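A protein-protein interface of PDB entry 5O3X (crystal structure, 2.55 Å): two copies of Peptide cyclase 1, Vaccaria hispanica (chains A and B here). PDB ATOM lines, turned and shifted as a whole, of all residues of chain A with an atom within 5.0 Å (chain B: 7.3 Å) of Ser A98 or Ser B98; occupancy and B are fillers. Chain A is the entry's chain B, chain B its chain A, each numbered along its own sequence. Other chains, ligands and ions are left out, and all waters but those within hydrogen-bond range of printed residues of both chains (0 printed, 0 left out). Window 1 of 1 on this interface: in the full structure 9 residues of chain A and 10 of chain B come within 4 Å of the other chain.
The side-chain amide nitrogen (ND2) of Asn B78 sits at hydrogen-bond distance from the backbone carbonyl oxygen (O) of Leu A100, 3.2 Å away. The side-chain hydroxyl (OG) of Ser B98 is in hydrogen-bond range of the side-chain hydroxyl (OG) of Ser A98, at 2.6 Å. O of Leu B100 is in hydrogen-bond range of ND2 of Asn A78, at 2.9 Å.
The backbone NH (N) of Ser B98 is in hydrogen-bond range of the side-chain amide oxygen (OE1) of Gln B101, 2.8 Å away. The backbone NH of Ser A98 lies within hydrogen-bond range of the side-chain amide oxygen of Gln A101 (2.8 Å).
Printed residues of chain B within 4 Å of Asn A78: Leu B100. Of the printed residues of chain B, Leu A100 touches Asn B78 (3.2 Å). Of the printed residues of chain A, Asn B78 touches Leu A100 (3.2 Å). Of the printed residues of chain A, Ser B98 touches Ser A98 (2.6 Å). Printed residues of chain A within 4 Å of Leu B100: Asn A78. Gln B103 touches none of the printed residues of chain A. Asn B123 touches none of the printed residues of chain A. The nearest residue of chain B that does not touch Ser A98 is Gln B101 (4.1 Å).
Of the 16 printed residues of chain B, 3 touch a printed residue of chain A. Among the printed residues, 3 pairs touch across the chains.
Asn A78 touches Leu B100, and with the chains exchanged Leu A100 touches Asn B78. Ser B98 touches its own counterpart, Ser A98. 9 positions are printed for both chains. Of the 3 pairs that touch across the chains among the printed residues, 3 have their exchanged pair printed and touching as well.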
ATOM      1  N   ASN A  78       7.040  -2.600   8.947  1.00  0.00           N
ATOM      2  CA  ASN A  78       8.235  -3.452   8.807  1.00  0.00           C
ATOM      3  C   ASN A  78       9.499  -2.708   9.262  1.00  0.00           C
ATOM      4  O   ASN A  78      10.362  -2.336   8.465  1.00  0.00           O
ATOM      5  CB  ASN A  78       8.361  -3.972   7.360  1.00  0.00           C
ATOM      6  CG  ASN A  78       9.321  -5.144   7.220  1.00  0.00           C
ATOM      7  OD1 ASN A  78       9.716  -5.770   8.200  1.00  0.00           O
ATOM      8  ND2 ASN A  78       9.685  -5.455   5.983  1.00  0.00           N
ATOM      9  N   PHE A  79       9.578  -2.498  10.573  1.00  0.00           N
ATOM     10  CA  PHE A  79      10.716  -1.878  11.245  1.00  0.00           C
ATOM     11  C   PHE A  79      10.907  -2.648  12.554  1.00  0.00           C
ATOM     12  O   PHE A  79       9.933  -3.203  13.066  1.00  0.00           O
ATOM     13  CB  PHE A  79      10.451  -0.383  11.508  1.00  0.00           C
ATOM     14  CG  PHE A  79       9.235  -0.104  12.382  1.00  0.00           C
ATOM     15  CD1 PHE A  79       9.361  -0.014  13.768  1.00  0.00           C
ATOM     16  CD2 PHE A  79       7.967   0.092  11.823  1.00  0.00           C
ATOM     17  CE1 PHE A  79       8.255   0.239  14.580  1.00  0.00           C
ATOM     18  CE2 PHE A  79       6.857   0.344  12.630  1.00  0.00           C
ATOM     19  CZ  PHE A  79       7.000   0.418  14.009  1.00  0.00           C
ATOM     20  N   PRO A  80      12.142  -2.702  13.094  1.00  0.00           N
ATOM     21  CA  PRO A  80      12.286  -3.363  14.399  1.00  0.00           C
ATOM     22  C   PRO A  80      11.553  -2.647  15.540  1.00  0.00           C
ATOM     23  O   PRO A  80      11.570  -1.416  15.620  1.00  0.00           O
ATOM     24  CB  PRO A  80      13.798  -3.365  14.649  1.00  0.00           C
ATOM     25  CG  PRO A  80      14.401  -3.270  13.297  1.00  0.00           C
ATOM     26  CD  PRO A  80      13.451  -2.425  12.479  1.00  0.00           C
ATOM     27  N   TYR A  96      11.470  -8.666  21.387  1.00  0.00           N
ATOM     28  CA  TYR A  96      11.928  -8.071  20.126  1.00  0.00           C
ATOM     29  C   TYR A  96      11.081  -8.591  18.939  1.00  0.00           C
ATOM     30  O   TYR A  96      10.489  -9.676  18.998  1.00  0.00           O
ATOM     31  CB  TYR A  96      13.415  -8.371  19.912  1.00  0.00           C
ATOM     32  CG  TYR A  96      13.995  -7.849  18.614  1.00  0.00           C
ATOM     33  CD1 TYR A  96      14.402  -6.533  18.496  1.00  0.00           C
ATOM     34  CD2 TYR A  96      14.149  -8.690  17.502  1.00  0.00           C
ATOM     35  CE1 TYR A  96      14.935  -6.043  17.303  1.00  0.00           C
ATOM     36  CE2 TYR A  96      14.674  -8.218  16.303  1.00  0.00           C
ATOM     37  CZ  TYR A  96      15.062  -6.894  16.204  1.00  0.00           C
ATOM     38  OH  TYR A  96      15.592  -6.413  15.015  1.00  0.00           O
ATOM     39  N   ASN A  97      11.014  -7.791  17.882  1.00  0.00           N
ATOM     40  CA  ASN A  97      10.390  -8.195  16.628  1.00  0.00           C
ATOM     41  C   ASN A  97      11.063  -7.433  15.497  1.00  0.00           C
ATOM     42  O   ASN A  97      11.051  -6.214  15.507  1.00  0.00           O
ATOM     43  CB  ASN A  97       8.887  -7.888  16.659  1.00  0.00           C
ATOM     44  CG  ASN A  97       8.129  -8.538  15.517  1.00  0.00           C
ATOM     45  OD1 ASN A  97       8.428  -8.313  14.350  1.00  0.00           O
ATOM     46  ND2 ASN A  97       7.124  -9.328  15.854  1.00  0.00           N
ATOM     47  N   SER A  98      11.630  -8.144  14.523  1.00  0.00           N
ATOM     48  CA  SER A  98      12.291  -7.501  13.396  1.00  0.00           C
ATOM     49  C   SER A  98      11.334  -6.659  12.542  1.00  0.00           C
ATOM     50  O   SER A  98      11.790  -5.778  11.810  1.00  0.00           O
ATOM     51  CB  SER A  98      13.001  -8.539  12.519  1.00  0.00           C
ATOM     52  OG  SER A  98      12.083  -9.441  11.937  1.00  0.00           O
ATOM     53  N   GLY A  99      10.027  -6.931  12.624  1.00  0.00           N
ATOM     54  CA  GLY A  99       9.007  -6.080  12.011  1.00  0.00           C
ATOM     55  C   GLY A  99       7.732  -6.803  11.608  1.00  0.00           C
ATOM     56  O   GLY A  99       6.639  -6.349  11.924  1.00  0.00           O
ATOM     57  N   LEU A 100       7.873  -7.918  10.897  1.00  0.00           N
ATOM     58  CA  LEU A 100       6.734  -8.714  10.429  1.00  0.00           C
ATOM     59  C   LEU A 100       6.856 -10.176  10.851  1.00  0.00           C
ATOM     60  O   LEU A 100       6.430 -11.082  10.133  1.00  0.00           O
ATOM     61  CB  LEU A 100       6.613  -8.615   8.900  1.00  0.00           C
ATOM     62  CG  LEU A 100       6.401  -7.222   8.317  1.00  0.00           C
ATOM     63  CD1 LEU A 100       6.531  -7.275   6.796  1.00  0.00           C
ATOM     64  CD2 LEU A 100       5.053  -6.646   8.748  1.00  0.00           C
ATOM     65  N   GLN A 101       7.429 -10.420  12.030  1.00  0.00           N
ATOM     66  CA  GLN A 101       7.439 -11.757  12.603  1.00  0.00           C
ATOM     67  C   GLN A 101       6.060 -11.963  13.205  1.00  0.00           C
ATOM     68  O   GLN A 101       5.500 -11.045  13.811  1.00  0.00           O
ATOM     69  CB  GLN A 101       8.529 -11.894  13.655  1.00  0.00           C
ATOM     70  CG  GLN A 101       9.933 -11.602  13.144  1.00  0.00           C
ATOM     71  CD  GLN A 101      11.017 -11.882  14.173  1.00  0.00           C
ATOM     72  OE1 GLN A 101      11.529 -10.969  14.817  1.00  0.00           O
ATOM     73  NE2 GLN A 101      11.376 -13.146  14.327  1.00  0.00           N
ATOM     74  N   VAL B  77       7.133 -17.663   2.720  1.00  0.00           N
ATOM     75  CA  VAL B  77       8.466 -17.049   2.732  1.00  0.00           C
ATOM     76  C   VAL B  77       8.880 -16.552   4.133  1.00  0.00           C
ATOM     77  O   VAL B  77      10.056 -16.233   4.348  1.00  0.00           O
ATOM     78  CB  VAL B  77       8.542 -15.913   1.673  1.00  0.00           C
ATOM     79  CG1 VAL B  77       9.853 -15.137   1.717  1.00  0.00           C
ATOM     80  CG2 VAL B  77       8.370 -16.491   0.274  1.00  0.00           C
ATOM     81  N   ASN B  78       7.947 -16.502   5.091  1.00  0.00           N
ATOM     82  CA  ASN B  78       8.233 -15.926   6.415  1.00  0.00           C
ATOM     83  C   ASN B  78       8.880 -16.962   7.352  1.00  0.00           C
ATOM     84  O   ASN B  78       8.272 -17.439   8.310  1.00  0.00           O
ATOM     85  CB  ASN B  78       6.967 -15.296   7.024  1.00  0.00           C
ATOM     86  CG  ASN B  78       7.266 -14.356   8.193  1.00  0.00           C
ATOM     87  OD1 ASN B  78       8.408 -13.938   8.423  1.00  0.00           O
ATOM     88  ND2 ASN B  78       6.221 -14.006   8.930  1.00  0.00           N
ATOM     89  N   PHE B  79      10.129 -17.294   7.033  1.00  0.00           N
ATOM     90  CA  PHE B  79      10.959 -18.214   7.805  1.00  0.00           C
ATOM     91  C   PHE B  79      12.378 -17.637   7.764  1.00  0.00           C
ATOM     92  O   PHE B  79      12.706 -16.928   6.817  1.00  0.00           O
ATOM     93  CB  PHE B  79      10.912 -19.638   7.200  1.00  0.00           C
ATOM     94  CG  PHE B  79      11.399 -19.729   5.765  1.00  0.00           C
ATOM     95  CD1 PHE B  79      12.743 -19.954   5.473  1.00  0.00           C
ATOM     96  CD2 PHE B  79      10.512 -19.598   4.696  1.00  0.00           C
ATOM     97  CE1 PHE B  79      13.197 -20.040   4.158  1.00  0.00           C
ATOM     98  CE2 PHE B  79      10.964 -19.686   3.374  1.00  0.00           C
ATOM     99  CZ  PHE B  79      12.305 -19.908   3.107  1.00  0.00           C
ATOM    100  N   PRO B  80      13.219 -17.918   8.779  1.00  0.00           N
ATOM    101  CA  PRO B  80      14.606 -17.430   8.679  1.00  0.00           C
ATOM    102  C   PRO B  80      15.406 -18.038   7.520  1.00  0.00           C
ATOM    103  O   PRO B  80      15.315 -19.236   7.266  1.00  0.00           O
ATOM    104  CB  PRO B  80      15.223 -17.827  10.029  1.00  0.00           C
ATOM    105  CG  PRO B  80      14.065 -17.939  10.952  1.00  0.00           C
ATOM    106  CD  PRO B  80      12.927 -18.450  10.121  1.00  0.00           C
ATOM    107  N   ARG B  81      16.159 -17.187   6.831  1.00  0.00           N
ATOM    108  CA  ARG B  81      17.089 -17.580   5.780  1.00  0.00           C
ATOM    109  C   ARG B  81      18.498 -17.145   6.176  1.00  0.00           C
ATOM    110  O   ARG B  81      18.713 -16.010   6.643  1.00  0.00           O
ATOM    111  CB  ARG B  81      16.684 -16.925   4.453  1.00  0.00           C
ATOM    112  CG  ARG B  81      15.567 -17.682   3.746  1.00  0.00           C
ATOM    113  CD  ARG B  81      15.118 -17.016   2.458  1.00  0.00           C
ATOM    114  NE  ARG B  81      14.224 -15.903   2.771  1.00  0.00           N
ATOM    115  CZ  ARG B  81      14.573 -14.624   2.879  1.00  0.00           C
ATOM    116  NH1 ARG B  81      15.837 -14.237   2.714  1.00  0.00           N
ATOM    117  NH2 ARG B  81      13.651 -13.717   3.179  1.00  0.00           N
ATOM    118  N   TYR B  96      21.944 -12.724   7.234  1.00  0.00           N
ATOM    119  CA  TYR B  96      20.743 -13.276   7.860  1.00  0.00           C
ATOM    120  C   TYR B  96      19.486 -12.466   7.475  1.00  0.00           C
ATOM    121  O   TYR B  96      19.571 -11.278   7.142  1.00  0.00           O
ATOM    122  CB  TYR B  96      20.930 -13.303   9.383  1.00  0.00           C
ATOM    123  CG  TYR B  96      19.740 -13.855  10.151  1.00  0.00           C
ATOM    124  CD1 TYR B  96      19.505 -15.237  10.238  1.00  0.00           C
ATOM    125  CD2 TYR B  96      18.817 -12.991  10.758  1.00  0.00           C
ATOM    126  CE1 TYR B  96      18.410 -15.726  10.930  1.00  0.00           C
ATOM    127  CE2 TYR B  96      17.719 -13.478  11.453  1.00  0.00           C
ATOM    128  CZ  TYR B  96      17.519 -14.842  11.546  1.00  0.00           C
ATOM    129  OH  TYR B  96      16.417 -15.314  12.239  1.00  0.00           O
ATOM    130  N   ASN B  97      18.331 -13.130   7.513  1.00  0.00           N
ATOM    131  CA  ASN B  97      17.037 -12.484   7.328  1.00  0.00           C
ATOM    132  C   ASN B  97      15.990 -13.283   8.099  1.00  0.00           C
ATOM    133  O   ASN B  97      15.807 -14.475   7.840  1.00  0.00           O
ATOM    134  CB  ASN B  97      16.689 -12.467   5.845  1.00  0.00           C
ATOM    135  CG  ASN B  97      15.499 -11.589   5.520  1.00  0.00           C
ATOM    136  OD1 ASN B  97      14.398 -11.760   6.066  1.00  0.00           O
ATOM    137  ND2 ASN B  97      15.714 -10.635   4.617  1.00  0.00           N
ATOM    138  N   SER B  98      15.291 -12.631   9.025  1.00  0.00           N
ATOM    139  CA  SER B  98      14.268 -13.297   9.815  1.00  0.00           C
ATOM    140  C   SER B  98      13.095 -13.845   8.969  1.00  0.00           C
ATOM    141  O   SER B  98      12.379 -14.741   9.425  1.00  0.00           O
ATOM    142  CB  SER B  98      13.750 -12.367  10.910  1.00  0.00           C
ATOM    143  OG  SER B  98      13.108 -11.238  10.354  1.00  0.00           O
ATOM    144  N   GLY B  99      12.908 -13.297   7.763  1.00  0.00           N
ATOM    145  CA  GLY B  99      11.944 -13.833   6.804  1.00  0.00           C
ATOM    146  C   GLY B  99      11.360 -12.811   5.846  1.00  0.00           C
ATOM    147  O   GLY B  99      11.330 -13.050   4.640  1.00  0.00           O
ATOM    148  N   LEU B 100      10.886 -11.685   6.382  1.00  0.00           N
ATOM    149  CA  LEU B 100      10.297 -10.617   5.568  1.00  0.00           C
ATOM    150  C   LEU B 100      10.975  -9.263   5.803  1.00  0.00           C
ATOM    151  O   LEU B 100      10.321  -8.226   5.693  1.00  0.00           O
ATOM    152  CB  LEU B 100       8.789 -10.525   5.844  1.00  0.00           C
ATOM    153  CG  LEU B 100       7.959 -11.784   5.551  1.00  0.00           C
ATOM    154  CD1 LEU B 100       6.545 -11.626   6.077  1.00  0.00           C
ATOM    155  CD2 LEU B 100       7.942 -12.086   4.064  1.00  0.00           C
ATOM    156  N   GLN B 101      12.271  -9.271   6.111  1.00  0.00           N
ATOM    157  CA  GLN B 101      13.023  -8.027   6.233  1.00  0.00           C
ATOM    158  C   GLN B 101      13.342  -7.569   4.818  1.00  0.00           C
ATOM    159  O   GLN B 101      13.673  -8.394   3.968  1.00  0.00           O
ATOM    160  CB  GLN B 101      14.319  -8.232   7.022  1.00  0.00           C
ATOM    161  CG  GLN B 101      14.100  -8.772   8.428  1.00  0.00           C
ATOM    162  CD  GLN B 101      15.386  -8.827   9.243  1.00  0.00           C
ATOM    163  OE1 GLN B 101      15.981  -9.892   9.397  1.00  0.00           O
ATOM    164  NE2 GLN B 101      15.829  -7.679   9.747  1.00  0.00           N
ATOM    165  N   GLN B 103      15.805  -6.091   3.452  1.00  0.00           N
ATOM    166  CA  GLN B 103      17.158  -6.492   3.056  1.00  0.00           C
ATOM    167  C   GLN B 103      17.776  -7.390   4.124  1.00  0.00           C
ATOM    168  O   GLN B 103      17.441  -7.295   5.307  1.00  0.00           O
ATOM    169  CB  GLN B 103      18.030  -5.265   2.844  1.00  0.00           C
ATOM    170  CG  GLN B 103      17.505  -4.287   1.792  1.00  0.00           C
ATOM    171  CD  GLN B 103      17.546  -4.825   0.372  1.00  0.00           C
ATOM    172  OE1 GLN B 103      18.295  -5.747   0.067  1.00  0.00           O
ATOM    173  NE2 GLN B 103      16.755  -4.221  -0.513  1.00  0.00           N
ATOM    174  N   ASN B 104      18.678  -8.260   3.685  1.00  0.00           N
ATOM    175  CA  ASN B 104      19.406  -9.171   4.568  1.00  0.00           C
ATOM    176  C   ASN B 104      20.369  -8.377   5.438  1.00  0.00           C
ATOM    177  O   ASN B 104      20.967  -7.396   4.986  1.00  0.00           O
ATOM    178  CB  ASN B 104      20.211 -10.198   3.758  1.00  0.00           C
ATOM    179  CG  ASN B 104      19.336 -11.176   2.984  1.00  0.00           C
ATOM    180  OD1 ASN B 104      18.111 -11.216   3.133  1.00  0.00           O
ATOM    181  ND2 ASN B 104      19.977 -12.015   2.197  1.00  0.00           N
ATOM    182  N   VAL B 105      20.507  -8.813   6.685  1.00  0.00           N
ATOM    183  CA  VAL B 105      21.366  -8.156   7.671  1.00  0.00           C
ATOM    184  C   VAL B 105      22.694  -8.892   7.713  1.00  0.00           C
ATOM    185  O   VAL B 105      22.704 -10.118   7.757  1.00  0.00           O
ATOM    186  CB  VAL B 105      20.710  -8.188   9.072  1.00  0.00           C
ATOM    187  CG1 VAL B 105      21.602  -7.500  10.105  1.00  0.00           C
ATOM    188  CG2 VAL B 105      19.312  -7.550   9.019  1.00  0.00           C
ATOM    189  N   ASP B 121      23.019  -3.261   9.266  1.00  0.00           N
ATOM    190  CA  ASP B 121      21.616  -3.501   8.934  1.00  0.00           C
ATOM    191  C   ASP B 121      21.117  -2.496   7.882  1.00  0.00           C
ATOM    192  O   ASP B 121      20.809  -1.367   8.215  1.00  0.00           O
ATOM    193  CB  ASP B 121      20.748  -3.440  10.196  1.00  0.00           C
ATOM    194  CG  ASP B 121      19.294  -3.855   9.933  1.00  0.00           C
ATOM    195  OD1 ASP B 121      18.945  -4.154   8.764  1.00  0.00           O
ATOM    196  OD2 ASP B 121      18.493  -3.868  10.898  1.00  0.00           O
ATOM    197  N   ASN B 123      18.265  -2.263   6.530  1.00  0.00           N
ATOM    198  CA  ASN B 123      16.881  -1.868   6.801  1.00  0.00           C
ATOM    199  C   ASN B 123      16.743  -0.550   7.584  1.00  0.00           C
ATOM    200  O   ASN B 123      15.690   0.086   7.544  1.00  0.00           O
ATOM    201  CB  ASN B 123      16.157  -2.990   7.539  1.00  0.00           C
ATOM    202  CG  ASN B 123      16.163  -4.288   6.761  1.00  0.00           C
ATOM    203  OD1 ASN B 123      15.623  -4.362   5.665  1.00  0.00           O
ATOM    204  ND2 ASN B 123      16.776  -5.320   7.325  1.00  0.00           N
